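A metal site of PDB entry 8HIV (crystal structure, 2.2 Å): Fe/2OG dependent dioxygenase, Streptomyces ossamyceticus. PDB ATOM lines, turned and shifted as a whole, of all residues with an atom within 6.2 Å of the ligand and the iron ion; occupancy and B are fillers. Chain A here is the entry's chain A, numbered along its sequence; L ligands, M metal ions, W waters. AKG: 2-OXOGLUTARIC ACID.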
ATOM      1  N   LEU A 118      22.927  11.109   3.583  1.00  0.00           N
ATOM      2  CA  LEU A 118      22.152  11.835   4.576  1.00  0.00           C
ATOM      3  C   LEU A 118      22.215  13.340   4.346  1.00  0.00           C
ATOM      4  O   LEU A 118      23.276  13.906   4.086  1.00  0.00           O
ATOM      5  CB  LEU A 118      22.692  11.509   5.972  1.00  0.00           C
ATOM      6  CG  LEU A 118      22.060  12.239   7.156  1.00  0.00           C
ATOM      7  CD1 LEU A 118      20.612  11.864   7.210  1.00  0.00           C
ATOM      8  CD2 LEU A 118      22.771  11.850   8.465  1.00  0.00           C
ATOM      9  N   GLN A 120      20.264  16.610   6.815  1.00  0.00           N
ATOM     10  CA  GLN A 120      19.738  16.708   8.167  1.00  0.00           C
ATOM     11  C   GLN A 120      19.298  18.136   8.473  1.00  0.00           C
ATOM     12  O   GLN A 120      19.886  19.100   7.984  1.00  0.00           O
ATOM     13  CB  GLN A 120      20.795  16.348   9.214  1.00  0.00           C
ATOM     14  CG  GLN A 120      21.028  14.886   9.417  1.00  0.00           C
ATOM     15  CD  GLN A 120      21.942  14.674  10.587  1.00  0.00           C
ATOM     16  OE1 GLN A 120      23.022  15.254  10.645  1.00  0.00           O
ATOM     17  NE2 GLN A 120      21.512  13.855  11.544  1.00  0.00           N
ATOM     18  N   THR A 182      16.290  15.990  15.677  1.00  0.00           N
ATOM     19  CA  THR A 182      17.054  15.937  14.430  1.00  0.00           C
ATOM     20  C   THR A 182      16.245  15.206  13.385  1.00  0.00           C
ATOM     21  O   THR A 182      15.755  14.097  13.655  1.00  0.00           O
ATOM     22  CB  THR A 182      18.394  15.232  14.681  1.00  0.00           C
ATOM     23  OG1 THR A 182      19.163  16.032  15.574  1.00  0.00           O
ATOM     24  CG2 THR A 182      19.184  15.031  13.380  1.00  0.00           C
ATOM     25  N   ASN A 184      16.151  13.614   9.449  1.00  0.00           N
ATOM     26  CA  ASN A 184      17.067  12.947   8.526  1.00  0.00           C
ATOM     27  C   ASN A 184      16.362  12.637   7.217  1.00  0.00           C
ATOM     28  O   ASN A 184      15.249  12.100   7.219  1.00  0.00           O
ATOM     29  CB  ASN A 184      17.577  11.613   9.076  1.00  0.00           C
ATOM     30  CG  ASN A 184      18.369  11.758  10.355  1.00  0.00           C
ATOM     31  OD1 ASN A 184      19.132  12.702  10.530  1.00  0.00           O
ATOM     32  ND2 ASN A 184      18.213  10.793  11.237  1.00  0.00           N
ATOM     33  N   TYR A 186      17.542  10.694   3.424  1.00  0.00           N
ATOM     34  CA  TYR A 186      18.604   9.996   2.687  1.00  0.00           C
ATOM     35  C   TYR A 186      18.352  10.198   1.198  1.00  0.00           C
ATOM     36  O   TYR A 186      17.320   9.775   0.677  1.00  0.00           O
ATOM     37  CB  TYR A 186      18.657   8.510   3.072  1.00  0.00           C
ATOM     38  CG  TYR A 186      18.977   8.361   4.552  1.00  0.00           C
ATOM     39  CD1 TYR A 186      17.961   8.462   5.507  1.00  0.00           C
ATOM     40  CD2 TYR A 186      20.301   8.227   4.986  1.00  0.00           C
ATOM     41  CE1 TYR A 186      18.256   8.407   6.876  1.00  0.00           C
ATOM     42  CE2 TYR A 186      20.608   8.154   6.326  1.00  0.00           C
ATOM     43  CZ  TYR A 186      19.585   8.243   7.278  1.00  0.00           C
ATOM     44  OH  TYR A 186      19.929   8.192   8.602  1.00  0.00           O
ATOM     45  N   LEU A 195      24.402   6.308   5.822  1.00  0.00           N
ATOM     46  CA  LEU A 195      25.096   6.985   6.907  1.00  0.00           C
ATOM     47  C   LEU A 195      26.133   5.996   7.425  1.00  0.00           C
ATOM     48  O   LEU A 195      25.786   4.851   7.737  1.00  0.00           O
ATOM     49  CB  LEU A 195      24.120   7.401   8.021  1.00  0.00           C
ATOM     50  CG  LEU A 195      24.707   8.035   9.285  1.00  0.00           C
ATOM     51  CD1 LEU A 195      25.562   9.282   8.964  1.00  0.00           C
ATOM     52  CD2 LEU A 195      23.571   8.420  10.232  1.00  0.00           C
ATOM     53  N   HIS A 198      29.073   4.630  13.036  1.00  0.00           N
ATOM     54  CA  HIS A 198      29.393   5.594  14.071  1.00  0.00           C
ATOM     55  C   HIS A 198      28.751   5.119  15.365  1.00  0.00           C
ATOM     56  O   HIS A 198      27.868   4.247  15.377  1.00  0.00           O
ATOM     57  CB  HIS A 198      28.916   7.002  13.699  1.00  0.00           C
ATOM     58  CG  HIS A 198      27.424   7.110  13.642  1.00  0.00           C
ATOM     59  ND1 HIS A 198      26.669   6.622  12.598  1.00  0.00           N
ATOM     60  CD2 HIS A 198      26.540   7.581  14.563  1.00  0.00           C
ATOM     61  CE1 HIS A 198      25.386   6.804  12.862  1.00  0.00           C
ATOM     62  NE2 HIS A 198      25.290   7.375  14.040  1.00  0.00           N
ATOM     63  N   LYS A 199      29.192   5.706  16.454  1.00  0.00           N
ATOM     64  CA  LYS A 199      28.480   5.633  17.710  1.00  0.00           C
ATOM     65  C   LYS A 199      27.952   7.033  18.005  1.00  0.00           C
ATOM     66  O   LYS A 199      28.620   8.032  17.699  1.00  0.00           O
ATOM     67  CB  LYS A 199      29.400   5.143  18.829  1.00  0.00           C
ATOM     68  CG  LYS A 199      30.034   3.783  18.555  1.00  0.00           C
ATOM     69  CD  LYS A 199      31.163   3.502  19.575  1.00  0.00           C
ATOM     70  CE  LYS A 199      31.727   2.084  19.439  1.00  0.00           C
ATOM     71  NZ  LYS A 199      32.931   1.906  20.329  1.00  0.00           N
ATOM     72  N   ASP A 200      26.751   7.118  18.569  1.00  0.00           N
ATOM     73  CA  ASP A 200      26.187   8.422  18.913  1.00  0.00           C
ATOM     74  C   ASP A 200      26.970   9.051  20.056  1.00  0.00           C
ATOM     75  O   ASP A 200      27.537   8.348  20.896  1.00  0.00           O
ATOM     76  CB  ASP A 200      24.710   8.286  19.311  1.00  0.00           C
ATOM     77  CG  ASP A 200      23.821   7.981  18.131  1.00  0.00           C
ATOM     78  OD1 ASP A 200      24.326   8.157  17.001  1.00  0.00           O
ATOM     79  OD2 ASP A 200      22.658   7.535  18.306  1.00  0.00           O
ATOM     80  N   THR A 205      19.504   7.971  22.759  1.00  0.00           N
ATOM     81  CA  THR A 205      18.883   8.297  21.493  1.00  0.00           C
ATOM     82  C   THR A 205      17.558   7.584  21.425  1.00  0.00           C
ATOM     83  O   THR A 205      17.485   6.390  21.688  1.00  0.00           O
ATOM     84  CB  THR A 205      19.756   7.847  20.315  1.00  0.00           C
ATOM     85  OG1 THR A 205      20.992   8.547  20.338  1.00  0.00           O
ATOM     86  CG2 THR A 205      19.022   8.084  18.999  1.00  0.00           C
ATOM     87  N   LEU A 207      14.951   6.943  18.471  1.00  0.00           N
ATOM     88  CA  LEU A 207      14.920   7.027  17.020  1.00  0.00           C
ATOM     89  C   LEU A 207      13.550   6.586  16.491  1.00  0.00           C
ATOM     90  O   LEU A 207      13.058   5.512  16.851  1.00  0.00           O
ATOM     91  CB  LEU A 207      16.022   6.165  16.407  1.00  0.00           C
ATOM     92  CG  LEU A 207      16.171   6.237  14.883  1.00  0.00           C
ATOM     93  CD1 LEU A 207      16.612   7.651  14.443  1.00  0.00           C
ATOM     94  CD2 LEU A 207      17.181   5.204  14.412  1.00  0.00           C
ATOM     95  N   ARG A 208      12.963   7.410  15.644  1.00  0.00           N
ATOM     96  CA  ARG A 208      11.721   7.085  14.970  1.00  0.00           C
ATOM     97  C   ARG A 208      12.055   6.787  13.518  1.00  0.00           C
ATOM     98  O   ARG A 208      12.365   7.698  12.735  1.00  0.00           O
ATOM     99  CB  ARG A 208      10.712   8.233  15.084  1.00  0.00           C
ATOM    100  CG  ARG A 208       9.247   7.850  14.827  1.00  0.00           C
ATOM    101  CD  ARG A 208       8.966   7.581  13.344  1.00  0.00           C
ATOM    102  NE  ARG A 208       7.560   7.696  12.966  1.00  0.00           N
ATOM    103  CZ  ARG A 208       6.647   6.757  13.166  1.00  0.00           C
ATOM    104  NH1 ARG A 208       6.993   5.615  13.757  1.00  0.00           N
ATOM    105  NH2 ARG A 208       5.394   6.950  12.768  1.00  0.00           N
ATOM    106  N   THR A 209      11.998   5.523  13.151  1.00  0.00           N
ATOM    107  CA  THR A 209      12.262   5.074  11.795  1.00  0.00           C
ATOM    108  C   THR A 209      11.119   4.161  11.387  1.00  0.00           C
ATOM    109  O   THR A 209      10.628   3.375  12.186  1.00  0.00           O
ATOM    110  CB  THR A 209      13.598   4.326  11.704  1.00  0.00           C
ATOM    111  OG1 THR A 209      13.821   3.963  10.335  1.00  0.00           O
ATOM    112  CG2 THR A 209      13.571   3.053  12.555  1.00  0.00           C
ATOM    113  N   GLY A 213      16.799  -0.044   6.684  1.00  0.00           N
ATOM    114  CA  GLY A 213      18.048   0.658   6.429  1.00  0.00           C
ATOM    115  C   GLY A 213      18.974   0.697   7.612  1.00  0.00           C
ATOM    116  O   GLY A 213      20.207   0.721   7.451  1.00  0.00           O
ATOM    117  N   LEU A 214      18.422   0.771   8.815  1.00  0.00           N
ATOM    118  CA  LEU A 214      19.285   0.842   9.990  1.00  0.00           C
ATOM    119  C   LEU A 214      19.935  -0.513  10.227  1.00  0.00           C
ATOM    120  O   LEU A 214      19.287  -1.554  10.106  1.00  0.00           O
ATOM    121  CB  LEU A 214      18.490   1.305  11.204  1.00  0.00           C
ATOM    122  CG  LEU A 214      19.254   1.462  12.512  1.00  0.00           C
ATOM    123  CD1 LEU A 214      20.348   2.562  12.476  1.00  0.00           C
ATOM    124  CD2 LEU A 214      18.234   1.748  13.612  1.00  0.00           C
ATOM    125  N   ASN A 235      18.923   3.622  21.750  1.00  0.00           N
ATOM    126  CA  ASN A 235      20.278   3.154  21.984  1.00  0.00           C
ATOM    127  C   ASN A 235      21.015   4.208  22.793  1.00  0.00           C
ATOM    128  O   ASN A 235      20.511   5.301  23.035  1.00  0.00           O
ATOM    129  CB  ASN A 235      21.022   2.857  20.673  1.00  0.00           C
ATOM    130  CG  ASN A 235      21.068   4.065  19.744  1.00  0.00           C
ATOM    131  OD1 ASN A 235      20.232   4.194  18.855  1.00  0.00           O
ATOM    132  ND2 ASN A 235      22.057   4.937  19.927  1.00  0.00           N
ATOM    133  N   HIS A 256      26.498   1.716  14.675  1.00  0.00           N
ATOM    134  CA  HIS A 256      25.373   1.505  13.761  1.00  0.00           C
ATOM    135  C   HIS A 256      25.577   2.357  12.510  1.00  0.00           C
ATOM    136  O   HIS A 256      26.462   3.212  12.447  1.00  0.00           O
ATOM    137  CB  HIS A 256      24.021   1.785  14.447  1.00  0.00           C
ATOM    138  CG  HIS A 256      23.940   3.149  15.052  1.00  0.00           C
ATOM    139  ND1 HIS A 256      24.676   3.528  16.158  1.00  0.00           N
ATOM    140  CD2 HIS A 256      23.197   4.234  14.722  1.00  0.00           C
ATOM    141  CE1 HIS A 256      24.414   4.789  16.463  1.00  0.00           C
ATOM    142  NE2 HIS A 256      23.498   5.226  15.624  1.00  0.00           N
ATOM    143  N   ARG A 257      24.749   2.115  11.516  1.00  0.00           N
ATOM    144  CA  ARG A 257      24.899   2.763  10.226  1.00  0.00           C
ATOM    145  C   ARG A 257      23.583   2.604   9.489  1.00  0.00           C
ATOM    146  O   ARG A 257      22.694   1.857   9.932  1.00  0.00           O
ATOM    147  CB  ARG A 257      26.053   2.140   9.421  1.00  0.00           C
ATOM    148  CG  ARG A 257      25.684   0.788   8.830  1.00  0.00           C
ATOM    149  CD  ARG A 257      26.911   0.033   8.314  1.00  0.00           C
ATOM    150  NE  ARG A 257      26.570  -1.273   7.746  1.00  0.00           N
ATOM    151  CZ  ARG A 257      27.459  -2.177   7.339  1.00  0.00           C
ATOM    152  NH1 ARG A 257      28.769  -1.931   7.443  1.00  0.00           N
ATOM    153  NH2 ARG A 257      27.042  -3.339   6.835  1.00  0.00           N
ATOM    154  N   VAL A 258      23.459   3.304   8.370  1.00  0.00           N
ATOM    155  CA  VAL A 258      22.292   3.196   7.495  1.00  0.00           C
ATOM    156  C   VAL A 258      22.814   2.766   6.141  1.00  0.00           C
ATOM    157  O   VAL A 258      23.702   3.435   5.573  1.00  0.00           O
ATOM    158  CB  VAL A 258      21.523   4.528   7.367  1.00  0.00           C
ATOM    159  CG1 VAL A 258      20.414   4.381   6.334  1.00  0.00           C
ATOM    160  CG2 VAL A 258      20.986   4.991   8.731  1.00  0.00           C
ATOM    161  N   ARG A 265      14.509   7.760   1.946  1.00  0.00           N
ATOM    162  CA  ARG A 265      14.166   7.313   3.282  1.00  0.00           C
ATOM    163  C   ARG A 265      14.245   8.556   4.150  1.00  0.00           C
ATOM    164  O   ARG A 265      15.006   9.476   3.870  1.00  0.00           O
ATOM    165  CB  ARG A 265      15.120   6.208   3.756  1.00  0.00           C
ATOM    166  CG  ARG A 265      14.909   5.632   5.172  1.00  0.00           C
ATOM    167  CD  ARG A 265      16.045   4.614   5.522  1.00  0.00           C
ATOM    168  NE  ARG A 265      15.903   4.035   6.864  1.00  0.00           N
ATOM    169  CZ  ARG A 265      16.406   4.591   7.960  1.00  0.00           C
ATOM    170  NH1 ARG A 265      17.087   5.725   7.874  1.00  0.00           N
ATOM    171  NH2 ARG A 265      16.262   4.008   9.144  1.00  0.00           N
ATOM    172  N   SER A 266      13.373   8.624   5.169  1.00  0.00           N
ATOM    173  CA  SER A 266      13.495   9.687   6.144  1.00  0.00           C
ATOM    174  C   SER A 266      13.243   9.102   7.520  1.00  0.00           C
ATOM    175  O   SER A 266      12.725   7.984   7.657  1.00  0.00           O
ATOM    176  CB  SER A 266      12.539  10.866   5.873  1.00  0.00           C
ATOM    177  OG  SER A 266      11.195  10.430   5.999  1.00  0.00           O
ATOM    178  N   SER A 267      13.640   9.865   8.527  1.00  0.00           N
ATOM    179  CA  SER A 267      13.527   9.469   9.918  1.00  0.00           C
ATOM    180  C   SER A 267      13.780  10.690  10.782  1.00  0.00           C
ATOM    181  O   SER A 267      14.150  11.756  10.276  1.00  0.00           O
ATOM    182  CB  SER A 267      14.505   8.346  10.270  1.00  0.00           C
ATOM    183  OG  SER A 267      15.851   8.823  10.229  1.00  0.00           O
ATOM    184  N   PHE A 268      13.590  10.532  12.091  1.00  0.00           N
ATOM    185  CA  PHE A 268      14.003  11.592  12.983  1.00  0.00           C
ATOM    186  C   PHE A 268      14.311  11.002  14.346  1.00  0.00           C
ATOM    187  O   PHE A 268      13.896   9.879  14.670  1.00  0.00           O
ATOM    188  CB  PHE A 268      12.956  12.717  13.077  1.00  0.00           C
ATOM    189  CG  PHE A 268      11.630  12.310  13.673  1.00  0.00           C
ATOM    190  CD1 PHE A 268      11.432  12.387  15.048  1.00  0.00           C
ATOM    191  CD2 PHE A 268      10.586  11.886  12.872  1.00  0.00           C
ATOM    192  CE1 PHE A 268      10.212  12.021  15.616  1.00  0.00           C
ATOM    193  CE2 PHE A 268       9.343  11.538  13.426  1.00  0.00           C
ATOM    194  CZ  PHE A 268       9.162  11.605  14.801  1.00  0.00           C
ATOM    195  N   PHE A 271      17.973  13.274  20.711  1.00  0.00           N
ATOM    196  CA  PHE A 271      19.284  12.945  21.246  1.00  0.00           C
ATOM    197  C   PHE A 271      19.489  13.722  22.541  1.00  0.00           C
ATOM    198  O   PHE A 271      19.267  14.933  22.578  1.00  0.00           O
ATOM    199  CB  PHE A 271      20.393  13.285  20.230  1.00  0.00           C
ATOM    200  CG  PHE A 271      20.287  12.518  18.916  1.00  0.00           C
ATOM    201  CD1 PHE A 271      19.321  12.854  17.973  1.00  0.00           C
ATOM    202  CD2 PHE A 271      21.145  11.467  18.638  1.00  0.00           C
ATOM    203  CE1 PHE A 271      19.222  12.155  16.762  1.00  0.00           C
ATOM    204  CE2 PHE A 271      21.063  10.756  17.441  1.00  0.00           C
ATOM    205  CZ  PHE A 271      20.096  11.092  16.498  1.00  0.00           C
HETATM  206  C1  AKG L   1      21.796   9.349  13.533  1.00  0.00           C
HETATM  207  O1  AKG L   1      22.823   9.419  14.263  1.00  0.00           O
HETATM  208  O2  AKG L   1      21.227  10.413  13.149  1.00  0.00           O
HETATM  209  C2  AKG L   1      21.253   8.057  13.108  1.00  0.00           C
HETATM  210  O5  AKG L   1      21.750   6.988  13.484  1.00  0.00           O
HETATM  211  C3  AKG L   1      20.066   8.030  12.177  1.00  0.00           C
HETATM  212  C4  AKG L   1      19.656   6.572  11.891  1.00  0.00           C
HETATM  213  C5  AKG L   1      18.455   6.505  10.953  1.00  0.00           C
HETATM  214  O3  AKG L   1      17.742   5.491  10.989  1.00  0.00           O
HETATM  215  O4  AKG L   1      18.230   7.442  10.159  1.00  0.00           O
HETATM  216 FE    FE M   1      23.230   7.379  15.154  1.00  0.00          FE
HETATM  217  O   HOH W   1      21.150   7.175  16.195  1.00  0.00           O
HETATM  218  O   HOH W   2      22.298  12.838  14.056  1.00  0.00           O
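The side-chain hydroxyl (OH) of Tyr 186 is in hydrogen-bond range of an oxygen (O4) of the ligand (2.4 Å).
The side-chain hydroxyl (OG) of Ser 267 sits at hydrogen-bond distance from an oxygen (O4) of the ligand (2.8 Å).
The guanidinium group (NH2) of Arg 265 is in salt-bridge range of an oxygen (O3) of the ligand (2.8 Å).
Merely in contact with the ligand: Gln 120 (3.8 Å), Asn 184 (3.5 Å), Leu 195 (3.7 Å), Leu 207 (3.5 Å), Val 258 (3.7 Å) and Phe 271 (3.6 Å).
Of the 24 residues printed, 12 come within 4 Å of the ligand.
The nearest printed residue that does not touch the ligand is Leu 214 (4.1 Å).
The iron ion is bound by NE2 of His 256 (2.2 Å).
The iron ion is bound by an oxygen (O1) of the ligand (2.3 Å).
The iron ion is bound by O5 of the ligand (2.3 Å).
The iron ion is bound by the side-chain carboxylate (OD1) of Asp 200 (2.3 Å).
Water W1 binds the iron ion, 2.3 Å away.
A ring nitrogen (NE2) of His 198 is bound to the iron ion (2.3 Å).
The side-chain carboxylate (OD2) of Asp 200 sits at hydrogen-bond distance from the side-chain amide nitrogen (ND2) of Asn 235, 3.1 Å away.
The side-chain hydroxyl (OG1) of Thr 209 lies within hydrogen-bond range of the guanidinium group (NH2) of Arg 265, 2.7 Å away.
The backbone NH of Val 258 lies within hydrogen-bond range of the backbone carbonyl oxygen of Leu 195 (2.9 Å).
OD1 of Asn 184 lies within hydrogen-bond range of NE2 of Gln 120.
OG1 of Thr 205 sits at hydrogen-bond distance from OD2 of Asp 200 (2.8 Å).
The backbone NH of Tyr 186 is in hydrogen-bond range of the backbone carbonyl oxygen of Arg 265 (2.8 Å).
N of Asn 184 lies within hydrogen-bond range of O of Ser 267, at 2.9 Å.
Of the 24 residues printed, 3 come within 4 Å of the iron ion.
Water W2 lies within hydrogen-bond range of an oxygen (O2) of the ligand and the side-chain amide nitrogen of Gln 120.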
